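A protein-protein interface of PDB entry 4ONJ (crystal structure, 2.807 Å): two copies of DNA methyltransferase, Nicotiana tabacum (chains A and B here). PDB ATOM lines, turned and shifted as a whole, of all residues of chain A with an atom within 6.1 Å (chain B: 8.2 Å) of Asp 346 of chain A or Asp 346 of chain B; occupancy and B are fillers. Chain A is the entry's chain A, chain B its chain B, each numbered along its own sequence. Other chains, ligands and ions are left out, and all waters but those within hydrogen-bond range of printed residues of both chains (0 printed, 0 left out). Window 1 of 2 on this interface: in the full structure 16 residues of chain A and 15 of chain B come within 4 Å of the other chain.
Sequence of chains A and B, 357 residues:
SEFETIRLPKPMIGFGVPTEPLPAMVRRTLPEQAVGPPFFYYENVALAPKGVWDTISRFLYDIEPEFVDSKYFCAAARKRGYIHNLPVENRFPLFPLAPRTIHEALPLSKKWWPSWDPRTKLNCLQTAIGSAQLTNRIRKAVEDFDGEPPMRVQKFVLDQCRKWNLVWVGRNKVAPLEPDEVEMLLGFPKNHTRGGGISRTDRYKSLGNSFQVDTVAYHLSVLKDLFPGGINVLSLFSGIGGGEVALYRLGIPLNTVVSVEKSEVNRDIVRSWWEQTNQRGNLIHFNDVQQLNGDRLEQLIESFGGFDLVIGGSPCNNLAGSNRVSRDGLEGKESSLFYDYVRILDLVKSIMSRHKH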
ATOM      1  N   TYR A  61     -20.868  -6.695  26.207  1.00  0.00           N
ATOM      2  CA  TYR A  61     -21.252  -6.792  27.614  1.00  0.00           C
ATOM      3  C   TYR A  61     -22.754  -6.937  27.840  1.00  0.00           C
ATOM      4  O   TYR A  61     -23.272  -6.515  28.873  1.00  0.00           O
ATOM      5  CB  TYR A  61     -20.709  -5.590  28.393  1.00  0.00           C
ATOM      6  CG  TYR A  61     -19.268  -5.285  28.066  1.00  0.00           C
ATOM      7  CD1 TYR A  61     -18.249  -6.132  28.482  1.00  0.00           C
ATOM      8  CD2 TYR A  61     -18.924  -4.159  27.330  1.00  0.00           C
ATOM      9  CE1 TYR A  61     -16.930  -5.864  28.181  1.00  0.00           C
ATOM     10  CE2 TYR A  61     -17.606  -3.882  27.023  1.00  0.00           C
ATOM     11  CZ  TYR A  61     -16.612  -4.739  27.452  1.00  0.00           C
ATOM     12  OH  TYR A  61     -15.296  -4.473  27.152  1.00  0.00           O
ATOM     13  N   TYR A 341     -13.374  -3.826  16.850  1.00  0.00           N
ATOM     14  CA  TYR A 341     -13.862  -2.795  17.745  1.00  0.00           C
ATOM     15  C   TYR A 341     -13.839  -3.369  19.157  1.00  0.00           C
ATOM     16  O   TYR A 341     -13.296  -2.763  20.082  1.00  0.00           O
ATOM     17  CB  TYR A 341     -15.284  -2.365  17.361  1.00  0.00           C
ATOM     18  CG  TYR A 341     -15.852  -1.316  18.278  1.00  0.00           C
ATOM     19  CD1 TYR A 341     -15.686   0.035  18.006  1.00  0.00           C
ATOM     20  CD2 TYR A 341     -16.548  -1.674  19.425  1.00  0.00           C
ATOM     21  CE1 TYR A 341     -16.201   1.001  18.851  1.00  0.00           C
ATOM     22  CE2 TYR A 341     -17.063  -0.720  20.274  1.00  0.00           C
ATOM     23  CZ  TYR A 341     -16.887   0.613  19.983  1.00  0.00           C
ATOM     24  OH  TYR A 341     -17.404   1.558  20.834  1.00  0.00           O
ATOM     25  N   VAL A 342     -14.425  -4.553  19.306  1.00  0.00           N
ATOM     26  CA  VAL A 342     -14.466  -5.237  20.594  1.00  0.00           C
ATOM     27  C   VAL A 342     -13.058  -5.503  21.110  1.00  0.00           C
ATOM     28  O   VAL A 342     -12.786  -5.333  22.292  1.00  0.00           O
ATOM     29  CB  VAL A 342     -15.232  -6.571  20.503  1.00  0.00           C
ATOM     30  CG1 VAL A 342     -15.451  -7.149  21.893  1.00  0.00           C
ATOM     31  CG2 VAL A 342     -16.561  -6.367  19.799  1.00  0.00           C
ATOM     32  N   ARG A 343     -12.163  -5.900  20.211  1.00  0.00           N
ATOM     33  CA  ARG A 343     -10.778  -6.193  20.572  1.00  0.00           C
ATOM     34  C   ARG A 343     -10.018  -4.971  21.076  1.00  0.00           C
ATOM     35  O   ARG A 343      -9.191  -5.068  21.980  1.00  0.00           O
ATOM     36  CB  ARG A 343     -10.032  -6.786  19.378  1.00  0.00           C
ATOM     37  CG  ARG A 343      -8.588  -7.141  19.676  1.00  0.00           C
ATOM     38  CD  ARG A 343      -7.822  -7.465  18.411  1.00  0.00           C
ATOM     39  NE  ARG A 343      -7.728  -6.308  17.527  1.00  0.00           N
ATOM     40  CZ  ARG A 343      -6.810  -5.354  17.642  1.00  0.00           C
ATOM     41  NH1 ARG A 343      -5.905  -5.414  18.609  1.00  0.00           N
ATOM     42  NH2 ARG A 343      -6.799  -4.337  16.793  1.00  0.00           N
ATOM     43  N   ILE A 344     -10.283  -3.821  20.473  1.00  0.00           N
ATOM     44  CA  ILE A 344      -9.573  -2.610  20.846  1.00  0.00           C
ATOM     45  C   ILE A 344     -10.172  -2.008  22.111  1.00  0.00           C
ATOM     46  O   ILE A 344      -9.449  -1.477  22.949  1.00  0.00           O
ATOM     47  CB  ILE A 344      -9.563  -1.598  19.693  1.00  0.00           C
ATOM     48  CG1 ILE A 344      -8.727  -2.148  18.541  1.00  0.00           C
ATOM     49  CG2 ILE A 344      -9.005  -0.259  20.144  1.00  0.00           C
ATOM     50  CD1 ILE A 344      -8.564  -1.190  17.418  1.00  0.00           C
ATOM     51  N   LEU A 345     -11.490  -2.129  22.250  1.00  0.00           N
ATOM     52  CA  LEU A 345     -12.208  -1.562  23.397  1.00  0.00           C
ATOM     53  C   LEU A 345     -11.661  -2.025  24.758  1.00  0.00           C
ATOM     54  O   LEU A 345     -11.461  -1.208  25.658  1.00  0.00           O
ATOM     55  CB  LEU A 345     -13.705  -1.876  23.302  1.00  0.00           C
ATOM     56  CG  LEU A 345     -14.549  -1.446  24.512  1.00  0.00           C
ATOM     57  CD1 LEU A 345     -14.329   0.021  24.857  1.00  0.00           C
ATOM     58  CD2 LEU A 345     -16.024  -1.717  24.270  1.00  0.00           C
ATOM     59  N   ASP A 346     -11.437  -3.337  24.867  1.00  0.00           N
ATOM     60  CA  ASP A 346     -11.041  -3.987  26.111  1.00  0.00           C
ATOM     61  C   ASP A 346      -9.526  -4.020  26.320  1.00  0.00           C
ATOM     62  O   ASP A 346      -9.054  -4.122  27.450  1.00  0.00           O
ATOM     63  CB  ASP A 346     -11.643  -5.404  26.197  1.00  0.00           C
ATOM     64  CG  ASP A 346     -11.609  -6.139  24.864  1.00  0.00           C
ATOM     65  OD1 ASP A 346     -10.745  -5.805  24.037  1.00  0.00           O
ATOM     66  OD2 ASP A 346     -12.451  -7.041  24.639  1.00  0.00           O
ATOM     67  N   LEU A 347      -8.771  -3.942  25.227  1.00  0.00           N
ATOM     68  CA  LEU A 347      -7.338  -3.745  25.335  1.00  0.00           C
ATOM     69  C   LEU A 347      -7.189  -2.436  26.090  1.00  0.00           C
ATOM     70  O   LEU A 347      -6.559  -2.386  27.142  1.00  0.00           O
ATOM     71  CB  LEU A 347      -6.677  -3.657  23.959  1.00  0.00           C
ATOM     72  CG  LEU A 347      -6.180  -4.989  23.388  1.00  0.00           C
ATOM     73  CD1 LEU A 347      -5.485  -4.795  22.042  1.00  0.00           C
ATOM     74  CD2 LEU A 347      -5.255  -5.685  24.373  1.00  0.00           C
ATOM     75  N   VAL A 348      -7.837  -1.398  25.568  1.00  0.00           N
ATOM     76  CA  VAL A 348      -7.890  -0.100  26.224  1.00  0.00           C
ATOM     77  C   VAL A 348      -8.465  -0.207  27.635  1.00  0.00           C
ATOM     78  O   VAL A 348      -7.880   0.295  28.595  1.00  0.00           O
ATOM     79  CB  VAL A 348      -8.728   0.903  25.411  1.00  0.00           C
ATOM     80  CG1 VAL A 348      -9.040   2.141  26.239  1.00  0.00           C
ATOM     81  CG2 VAL A 348      -8.002   1.278  24.127  1.00  0.00           C
ATOM     82  N   LYS A 349      -9.609  -0.869  27.747  1.00  0.00           N
ATOM     83  CA  LYS A 349     -10.312  -0.999  29.015  1.00  0.00           C
ATOM     84  C   LYS A 349      -9.501  -1.780  30.052  1.00  0.00           C
ATOM     85  O   LYS A 349      -9.564  -1.491  31.248  1.00  0.00           O
ATOM     86  CB  LYS A 349     -11.665  -1.664  28.779  1.00  0.00           C
ATOM     87  CG  LYS A 349     -12.476  -1.899  30.019  1.00  0.00           C
ATOM     88  CD  LYS A 349     -13.820  -2.477  29.657  1.00  0.00           C
ATOM     89  CE  LYS A 349     -14.433  -3.135  30.861  1.00  0.00           C
ATOM     90  NZ  LYS A 349     -14.643  -2.157  31.966  1.00  0.00           N
ATOM     91  N   SER A 350      -8.736  -2.763  29.590  1.00  0.00           N
ATOM     92  CA  SER A 350      -7.890  -3.550  30.485  1.00  0.00           C
ATOM     93  C   SER A 350      -6.676  -2.754  30.948  1.00  0.00           C
ATOM     94  O   SER A 350      -6.365  -2.724  32.137  1.00  0.00           O
ATOM     95  CB  SER A 350      -7.442  -4.851  29.816  1.00  0.00           C
ATOM     96  OG  SER A 350      -6.470  -5.521  30.592  1.00  0.00           O
ATOM     97  N   ILE A 351      -5.994  -2.115  29.999  1.00  0.00           N
ATOM     98  CA  ILE A 351      -4.824  -1.292  30.299  1.00  0.00           C
ATOM     99  C   ILE A 351      -5.163  -0.172  31.279  1.00  0.00           C
ATOM    100  O   ILE A 351      -4.355   0.188  32.131  1.00  0.00           O
ATOM    101  CB  ILE A 351      -4.229  -0.663  29.017  1.00  0.00           C
ATOM    102  CG1 ILE A 351      -3.747  -1.745  28.054  1.00  0.00           C
ATOM    103  CG2 ILE A 351      -3.071   0.268  29.351  1.00  0.00           C
ATOM    104  CD1 ILE A 351      -3.180  -1.191  26.765  1.00  0.00           C
ATOM    105  N   GLN B  33      -0.643  -7.690  29.254  1.00  0.00           N
ATOM    106  CA  GLN B  33      -1.998  -8.137  28.983  1.00  0.00           C
ATOM    107  C   GLN B  33      -2.098  -9.648  28.895  1.00  0.00           C
ATOM    108  O   GLN B  33      -3.095 -10.234  29.304  1.00  0.00           O
ATOM    109  CB  GLN B  33      -2.505  -7.529  27.677  1.00  0.00           C
ATOM    110  CG  GLN B  33      -3.048  -6.143  27.844  1.00  0.00           C
ATOM    111  CD  GLN B  33      -3.992  -6.046  29.018  1.00  0.00           C
ATOM    112  OE1 GLN B  33      -3.803  -5.260  29.937  1.00  0.00           O
ATOM    113  NE2 GLN B  33      -5.042  -6.888  28.987  1.00  0.00           N
ATOM    114  N   PRO B  38      -6.015 -15.874  34.121  1.00  0.00           N
ATOM    115  CA  PRO B  38      -5.814 -17.319  33.978  1.00  0.00           C
ATOM    116  C   PRO B  38      -4.795 -17.655  32.901  1.00  0.00           C
ATOM    117  O   PRO B  38      -4.497 -16.821  32.047  1.00  0.00           O
ATOM    118  CB  PRO B  38      -7.190 -17.803  33.527  1.00  0.00           C
ATOM    119  CG  PRO B  38      -7.713 -16.669  32.718  1.00  0.00           C
ATOM    120  CD  PRO B  38      -7.219 -15.419  33.402  1.00  0.00           C
ATOM    121  N   PHE B  59      -5.680 -11.473  17.835  1.00  0.00           N
ATOM    122  CA  PHE B  59      -6.738 -11.383  18.832  1.00  0.00           C
ATOM    123  C   PHE B  59      -6.335 -11.968  20.181  1.00  0.00           C
ATOM    124  O   PHE B  59      -7.030 -11.781  21.180  1.00  0.00           O
ATOM    125  CB  PHE B  59      -8.008 -12.058  18.313  1.00  0.00           C
ATOM    126  CG  PHE B  59      -8.809 -11.197  17.385  1.00  0.00           C
ATOM    127  CD1 PHE B  59      -8.362 -10.936  16.101  1.00  0.00           C
ATOM    128  CD2 PHE B  59     -10.008 -10.642  17.800  1.00  0.00           C
ATOM    129  CE1 PHE B  59      -9.096 -10.136  15.246  1.00  0.00           C
ATOM    130  CE2 PHE B  59     -10.748  -9.843  16.950  1.00  0.00           C
ATOM    131  CZ  PHE B  59     -10.291  -9.589  15.671  1.00  0.00           C
ATOM    132  N   LEU B  60      -5.211 -12.674  20.206  1.00  0.00           N
ATOM    133  CA  LEU B  60      -4.690 -13.216  21.453  1.00  0.00           C
ATOM    134  C   LEU B  60      -3.358 -12.570  21.826  1.00  0.00           C
ATOM    135  O   LEU B  60      -2.342 -13.250  21.987  1.00  0.00           O
ATOM    136  CB  LEU B  60      -4.570 -14.738  21.381  1.00  0.00           C
ATOM    137  CG  LEU B  60      -5.907 -15.483  21.355  1.00  0.00           C
ATOM    138  CD1 LEU B  60      -5.704 -16.954  21.052  1.00  0.00           C
ATOM    139  CD2 LEU B  60      -6.647 -15.312  22.673  1.00  0.00           C
ATOM    140  N   TYR B  61      -3.384 -11.245  21.941  1.00  0.00           N
ATOM    141  CA  TYR B  61      -2.280 -10.465  22.495  1.00  0.00           C
ATOM    142  C   TYR B  61      -0.993 -10.551  21.680  1.00  0.00           C
ATOM    143  O   TYR B  61       0.102 -10.395  22.219  1.00  0.00           O
ATOM    144  CB  TYR B  61      -2.039 -10.860  23.954  1.00  0.00           C
ATOM    145  CG  TYR B  61      -3.331 -11.065  24.711  1.00  0.00           C
ATOM    146  CD1 TYR B  61      -4.172  -9.996  24.982  1.00  0.00           C
ATOM    147  CD2 TYR B  61      -3.718 -12.329  25.138  1.00  0.00           C
ATOM    148  CE1 TYR B  61      -5.359 -10.174  25.663  1.00  0.00           C
ATOM    149  CE2 TYR B  61      -4.907 -12.517  25.822  1.00  0.00           C
ATOM    150  CZ  TYR B  61      -5.722 -11.434  26.081  1.00  0.00           C
ATOM    151  OH  TYR B  61      -6.904 -11.605  26.758  1.00  0.00           O
ATOM    152  N   LEU B 297     -20.648 -16.367  33.842  1.00  0.00           N
ATOM    153  CA  LEU B 297     -19.230 -16.432  34.159  1.00  0.00           C
ATOM    154  C   LEU B 297     -18.922 -15.860  35.537  1.00  0.00           C
ATOM    155  O   LEU B 297     -18.054 -16.361  36.245  1.00  0.00           O
ATOM    156  CB  LEU B 297     -18.418 -15.699  33.091  1.00  0.00           C
ATOM    157  CG  LEU B 297     -17.883 -16.555  31.942  1.00  0.00           C
ATOM    158  CD1 LEU B 297     -17.073 -17.710  32.497  1.00  0.00           C
ATOM    159  CD2 LEU B 297     -18.999 -17.079  31.060  1.00  0.00           C
ATOM    160  N   VAL B 310      -8.031 -21.607  30.914  1.00  0.00           N
ATOM    161  CA  VAL B 310      -9.075 -21.595  29.903  1.00  0.00           C
ATOM    162  C   VAL B 310      -8.530 -22.286  28.663  1.00  0.00           C
ATOM    163  O   VAL B 310      -7.576 -21.813  28.049  1.00  0.00           O
ATOM    164  CB  VAL B 310      -9.521 -20.166  29.564  1.00  0.00           C
ATOM    165  CG1 VAL B 310     -10.535 -20.181  28.436  1.00  0.00           C
ATOM    166  CG2 VAL B 310     -10.104 -19.492  30.796  1.00  0.00           C
ATOM    167  N   TYR B 339     -14.068 -16.164  17.940  1.00  0.00           N
ATOM    168  CA  TYR B 339     -14.268 -14.873  18.587  1.00  0.00           C
ATOM    169  C   TYR B 339     -15.041 -15.027  19.894  1.00  0.00           C
ATOM    170  O   TYR B 339     -14.920 -14.199  20.795  1.00  0.00           O
ATOM    171  CB  TYR B 339     -14.972 -13.891  17.646  1.00  0.00           C
ATOM    172  CG  TYR B 339     -14.204 -13.627  16.369  1.00  0.00           C
ATOM    173  CD1 TYR B 339     -12.961 -13.007  16.399  1.00  0.00           C
ATOM    174  CD2 TYR B 339     -14.720 -13.999  15.134  1.00  0.00           C
ATOM    175  CE1 TYR B 339     -12.253 -12.766  15.237  1.00  0.00           C
ATOM    176  CE2 TYR B 339     -14.019 -13.761  13.965  1.00  0.00           C
ATOM    177  CZ  TYR B 339     -12.788 -13.145  14.022  1.00  0.00           C
ATOM    178  OH  TYR B 339     -12.088 -12.906  12.863  1.00  0.00           O
ATOM    179  N   ASP B 340     -15.826 -16.094  19.998  1.00  0.00           N
ATOM    180  CA  ASP B 340     -16.510 -16.397  21.250  1.00  0.00           C
ATOM    181  C   ASP B 340     -15.529 -16.897  22.307  1.00  0.00           C
ATOM    182  O   ASP B 340     -15.719 -16.663  23.498  1.00  0.00           O
ATOM    183  CB  ASP B 340     -17.641 -17.405  21.037  1.00  0.00           C
ATOM    184  CG  ASP B 340     -18.969 -16.734  20.746  1.00  0.00           C
ATOM    185  OD1 ASP B 340     -19.572 -16.181  21.690  1.00  0.00           O
ATOM    186  OD2 ASP B 340     -19.412 -16.759  19.578  1.00  0.00           O
ATOM    187  N   TYR B 341     -14.477 -17.580  21.867  1.00  0.00           N
ATOM    188  CA  TYR B 341     -13.420 -18.002  22.780  1.00  0.00           C
ATOM    189  C   TYR B 341     -12.691 -16.781  23.324  1.00  0.00           C
ATOM    190  O   TYR B 341     -12.522 -16.636  24.534  1.00  0.00           O
ATOM    191  CB  TYR B 341     -12.431 -18.937  22.080  1.00  0.00           C
ATOM    192  CG  TYR B 341     -11.228 -19.303  22.927  1.00  0.00           C
ATOM    193  CD1 TYR B 341     -11.263 -20.394  23.789  1.00  0.00           C
ATOM    194  CD2 TYR B 341     -10.055 -18.562  22.858  1.00  0.00           C
ATOM    195  CE1 TYR B 341     -10.163 -20.732  24.563  1.00  0.00           C
ATOM    196  CE2 TYR B 341      -8.954 -18.890  23.627  1.00  0.00           C
ATOM    197  CZ  TYR B 341      -9.012 -19.974  24.475  1.00  0.00           C
ATOM    198  OH  TYR B 341      -7.912 -20.294  25.236  1.00  0.00           O
ATOM    199  N   VAL B 342     -12.256 -15.913  22.414  1.00  0.00           N
ATOM    200  CA  VAL B 342     -11.585 -14.670  22.778  1.00  0.00           C
ATOM    201  C   VAL B 342     -12.462 -13.818  23.696  1.00  0.00           C
ATOM    202  O   VAL B 342     -11.980 -13.237  24.670  1.00  0.00           O
ATOM    203  CB  VAL B 342     -11.188 -13.864  21.523  1.00  0.00           C
ATOM    204  CG1 VAL B 342     -10.692 -12.479  21.900  1.00  0.00           C
ATOM    205  CG2 VAL B 342     -10.129 -14.614  20.735  1.00  0.00           C
ATOM    206  N   ARG B 343     -13.755 -13.762  23.393  1.00  0.00           N
ATOM    207  CA  ARG B 343     -14.695 -13.028  24.230  1.00  0.00           C
ATOM    208  C   ARG B 343     -14.705 -13.573  25.646  1.00  0.00           C
ATOM    209  O   ARG B 343     -14.490 -12.833  26.607  1.00  0.00           O
ATOM    210  CB  ARG B 343     -16.110 -13.100  23.662  1.00  0.00           C
ATOM    211  CG  ARG B 343     -17.144 -12.453  24.566  1.00  0.00           C
ATOM    212  CD  ARG B 343     -18.533 -12.541  23.973  1.00  0.00           C
ATOM    213  NE  ARG B 343     -18.919 -13.924  23.721  1.00  0.00           N
ATOM    214  CZ  ARG B 343     -19.432 -14.733  24.640  1.00  0.00           C
ATOM    215  NH1 ARG B 343     -19.618 -14.296  25.879  1.00  0.00           N
ATOM    216  NH2 ARG B 343     -19.756 -15.978  24.323  1.00  0.00           N
ATOM    217  N   ILE B 344     -14.964 -14.872  25.761  1.00  0.00           N
ATOM    218  CA  ILE B 344     -15.046 -15.539  27.053  1.00  0.00           C
ATOM    219  C   ILE B 344     -13.752 -15.369  27.841  1.00  0.00           C
ATOM    220  O   ILE B 344     -13.781 -15.060  29.032  1.00  0.00           O
ATOM    221  CB  ILE B 344     -15.374 -17.033  26.887  1.00  0.00           C
ATOM    222  CG1 ILE B 344     -16.813 -17.200  26.398  1.00  0.00           C
ATOM    223  CG2 ILE B 344     -15.174 -17.779  28.195  1.00  0.00           C
ATOM    224  CD1 ILE B 344     -17.180 -18.627  26.055  1.00  0.00           C
ATOM    225  N   LEU B 345     -12.622 -15.551  27.165  1.00  0.00           N
ATOM    226  CA  LEU B 345     -11.322 -15.375  27.800  1.00  0.00           C
ATOM    227  C   LEU B 345     -11.176 -13.969  28.370  1.00  0.00           C
ATOM    228  O   LEU B 345     -10.649 -13.793  29.462  1.00  0.00           O
ATOM    229  CB  LEU B 345     -10.181 -15.669  26.823  1.00  0.00           C
ATOM    230  CG  LEU B 345      -8.777 -15.463  27.401  1.00  0.00           C
ATOM    231  CD1 LEU B 345      -8.581 -16.320  28.650  1.00  0.00           C
ATOM    232  CD2 LEU B 345      -7.699 -15.757  26.367  1.00  0.00           C
ATOM    233  N   ASP B 346     -11.659 -12.971  27.636  1.00  0.00           N
ATOM    234  CA  ASP B 346     -11.568 -11.582  28.086  1.00  0.00           C
ATOM    235  C   ASP B 346     -12.456 -11.293  29.294  1.00  0.00           C
ATOM    236  O   ASP B 346     -12.069 -10.539  30.184  1.00  0.00           O
ATOM    237  CB  ASP B 346     -11.889 -10.616  26.945  1.00  0.00           C
ATOM    238  CG  ASP B 346     -10.712 -10.402  26.016  1.00  0.00           C
ATOM    239  OD1 ASP B 346      -9.560 -10.453  26.498  1.00  0.00           O
ATOM    240  OD2 ASP B 346     -10.935 -10.184  24.808  1.00  0.00           O
ATOM    241  N   LEU B 347     -13.644 -11.891  29.320  1.00  0.00           N
ATOM    242  CA  LEU B 347     -14.557 -11.722  30.446  1.00  0.00           C
ATOM    243  C   LEU B 347     -13.989 -12.334  31.722  1.00  0.00           C
ATOM    244  O   LEU B 347     -13.846 -11.645  32.732  1.00  0.00           O
ATOM    245  CB  LEU B 347     -15.922 -12.331  30.134  1.00  0.00           C
ATOM    246  CG  LEU B 347     -16.834 -11.500  29.233  1.00  0.00           C
ATOM    247  CD1 LEU B 347     -18.093 -12.275  28.889  1.00  0.00           C
ATOM    248  CD2 LEU B 347     -17.181 -10.185  29.908  1.00  0.00           C
ATOM    249  N   VAL B 348     -13.677 -13.630  31.660  1.00  0.00           N
ATOM    250  CA  VAL B 348     -13.071 -14.364  32.767  1.00  0.00           C
ATOM    251  C   VAL B 348     -11.877 -13.606  33.328  1.00  0.00           C
ATOM    252  O   VAL B 348     -11.728 -13.435  34.538  1.00  0.00           O
ATOM    253  CB  VAL B 348     -12.565 -15.745  32.298  1.00  0.00           C
ATOM    254  CG1 VAL B 348     -11.737 -16.417  33.383  1.00  0.00           C
ATOM    255  CG2 VAL B 348     -13.727 -16.627  31.873  1.00  0.00           C
ATOM    256  N   LYS B 349     -11.037 -13.143  32.414  1.00  0.00           N
ATOM    257  CA  LYS B 349      -9.818 -12.436  32.749  1.00  0.00           C
ATOM    258  C   LYS B 349     -10.130 -11.104  33.420  1.00  0.00           C
ATOM    259  O   LYS B 349      -9.449 -10.687  34.357  1.00  0.00           O
ATOM    260  CB  LYS B 349      -9.044 -12.198  31.465  1.00  0.00           C
ATOM    261  CG  LYS B 349      -7.579 -12.043  31.636  1.00  0.00           C
ATOM    262  CD  LYS B 349      -6.921 -12.007  30.281  1.00  0.00           C
ATOM    263  CE  LYS B 349      -5.455 -11.748  30.449  1.00  0.00           C
ATOM    264  NZ  LYS B 349      -5.228 -10.795  31.572  1.00  0.00           N
ATOM    265  N   SER B 350     -11.167 -10.436  32.930  1.00  0.00           N
ATOM    266  CA  SER B 350     -11.588  -9.159  33.487  1.00  0.00           C
ATOM    267  C   SER B 350     -12.178  -9.339  34.881  1.00  0.00           C
ATOM    268  O   SER B 350     -11.874  -8.574  35.796  1.00  0.00           O
ATOM    269  CB  SER B 350     -12.605  -8.485  32.563  1.00  0.00           C
ATOM    270  OG  SER B 350     -13.218  -7.372  33.192  1.00  0.00           O
ATOM    271  N   ILE B 351     -13.019 -10.356  35.036  1.00  0.00           N
ATOM    272  CA  ILE B 351     -13.689 -10.619  36.307  1.00  0.00           C
ATOM    273  C   ILE B 351     -12.709 -10.929  37.438  1.00  0.00           C
ATOM    274  O   ILE B 351     -12.813 -10.372  38.531  1.00  0.00           O
ATOM    275  CB  ILE B 351     -14.685 -11.787  36.181  1.00  0.00           C
ATOM    276  CG1 ILE B 351     -15.802 -11.427  35.200  1.00  0.00           C
ATOM    277  CG2 ILE B 351     -15.266 -12.147  37.539  1.00  0.00           C
ATOM    278  CD1 ILE B 351     -16.881 -12.481  35.095  1.00  0.00           C
ATOM    279  N   MET B 352     -11.757 -11.815  37.169  1.00  0.00           N
ATOM    280  CA  MET B 352     -10.794 -12.232  38.181  1.00  0.00           C
ATOM    281  C   MET B 352      -9.860 -11.103  38.606  1.00  0.00           C
ATOM    282  O   MET B 352      -9.321 -11.107  39.713  1.00  0.00           O
ATOM    283  CB  MET B 352      -9.976 -13.426  37.677  1.00  0.00           C
ATOM    284  CG  MET B 352     -10.782 -14.706  37.501  1.00  0.00           C
ATOM    285  SD  MET B 352      -9.843 -16.022  36.702  1.00  0.00           S
ATOM    286  CE  MET B 352      -8.460 -16.189  37.830  1.00  0.00           C
ATOM    287  N   SER B 353      -9.684 -10.126  37.728  1.00  0.00           N
ATOM    288  CA  SER B 353      -8.701  -9.072  37.949  1.00  0.00           C
ATOM    289  C   SER B 353      -9.156  -7.997  38.944  1.00  0.00           C
ATOM    290  O   SER B 353      -8.344  -7.188  39.393  1.00  0.00           O
ATOM    291  CB  SER B 353      -8.347  -8.428  36.617  1.00  0.00           C
ATOM    292  OG  SER B 353      -9.531  -8.051  35.941  1.00  0.00           O
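The side-chain carboxylate (OD2) of Asp 346 of chain A lies close to the side-chain carboxylate (OD2) of Asp 346 of chain B (3.5 Å).
The side-chain hydroxyl (OG) of Ser 350 of chain A lies within hydrogen-bond range of the side-chain amide nitrogen (NE2) of Gln 33 of chain B, 2.5 Å away.
The side-chain carboxylate (OD1) of Asp 346 of chain A lies close to the backbone carbonyl oxygen (O) of Val 342 of chain A, at 2.7 Å.
The side-chain carboxylate (OD1) of Asp 346 of chain A lies close to the backbone carbonyl oxygen (O) of Arg 343 of chain A (2.7 Å).
The backbone carbonyl oxygen (O) of Gln 33 of chain B sits close to the side-chain amino group (NZ) of Lys 349 of chain B (3.2 Å).
OD1 of Asp 346 of chain B sits at hydrogen-bond distance from OH of Tyr 61 of chain B (2.9 Å).
Among the printed residues, merely in contact across the chains: Arg 343 of chain A with Phe 59 of chain B (3.9 Å) and Ile 351 of chain A with Gln 33 of chain B (3.8 Å).
Asp 346 of chain A touches one residue of chain B.
Of chain A, only Asp 346 comes within 4 Å of Asp 346 of chain B.
Of the printed residues of chain B, Arg 343 of chain A touches Phe 59.
Printed residues of chain B within 4 Å of Ser 350 of chain A: Gln 33.
Ile 351 of chain B touches none of the printed residues of chain A.
Leu 345 of chain A touches none of the printed residues of chain B.
The nearest printed residue of chain B that does not touch Arg 343 of chain A is Asp 346 of chain B (5.8 Å).
Along chain A the printed residues that touch a printed residue of chain B span positions 343 to 351.
Asp 346 of chain A touches its own counterpart, Asp 346 of chain B.
12 positions are printed for both chains.
Of the 4 pairs that touch across the chains among the printed residues, 1 has its exchanged pair printed and touching as well.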
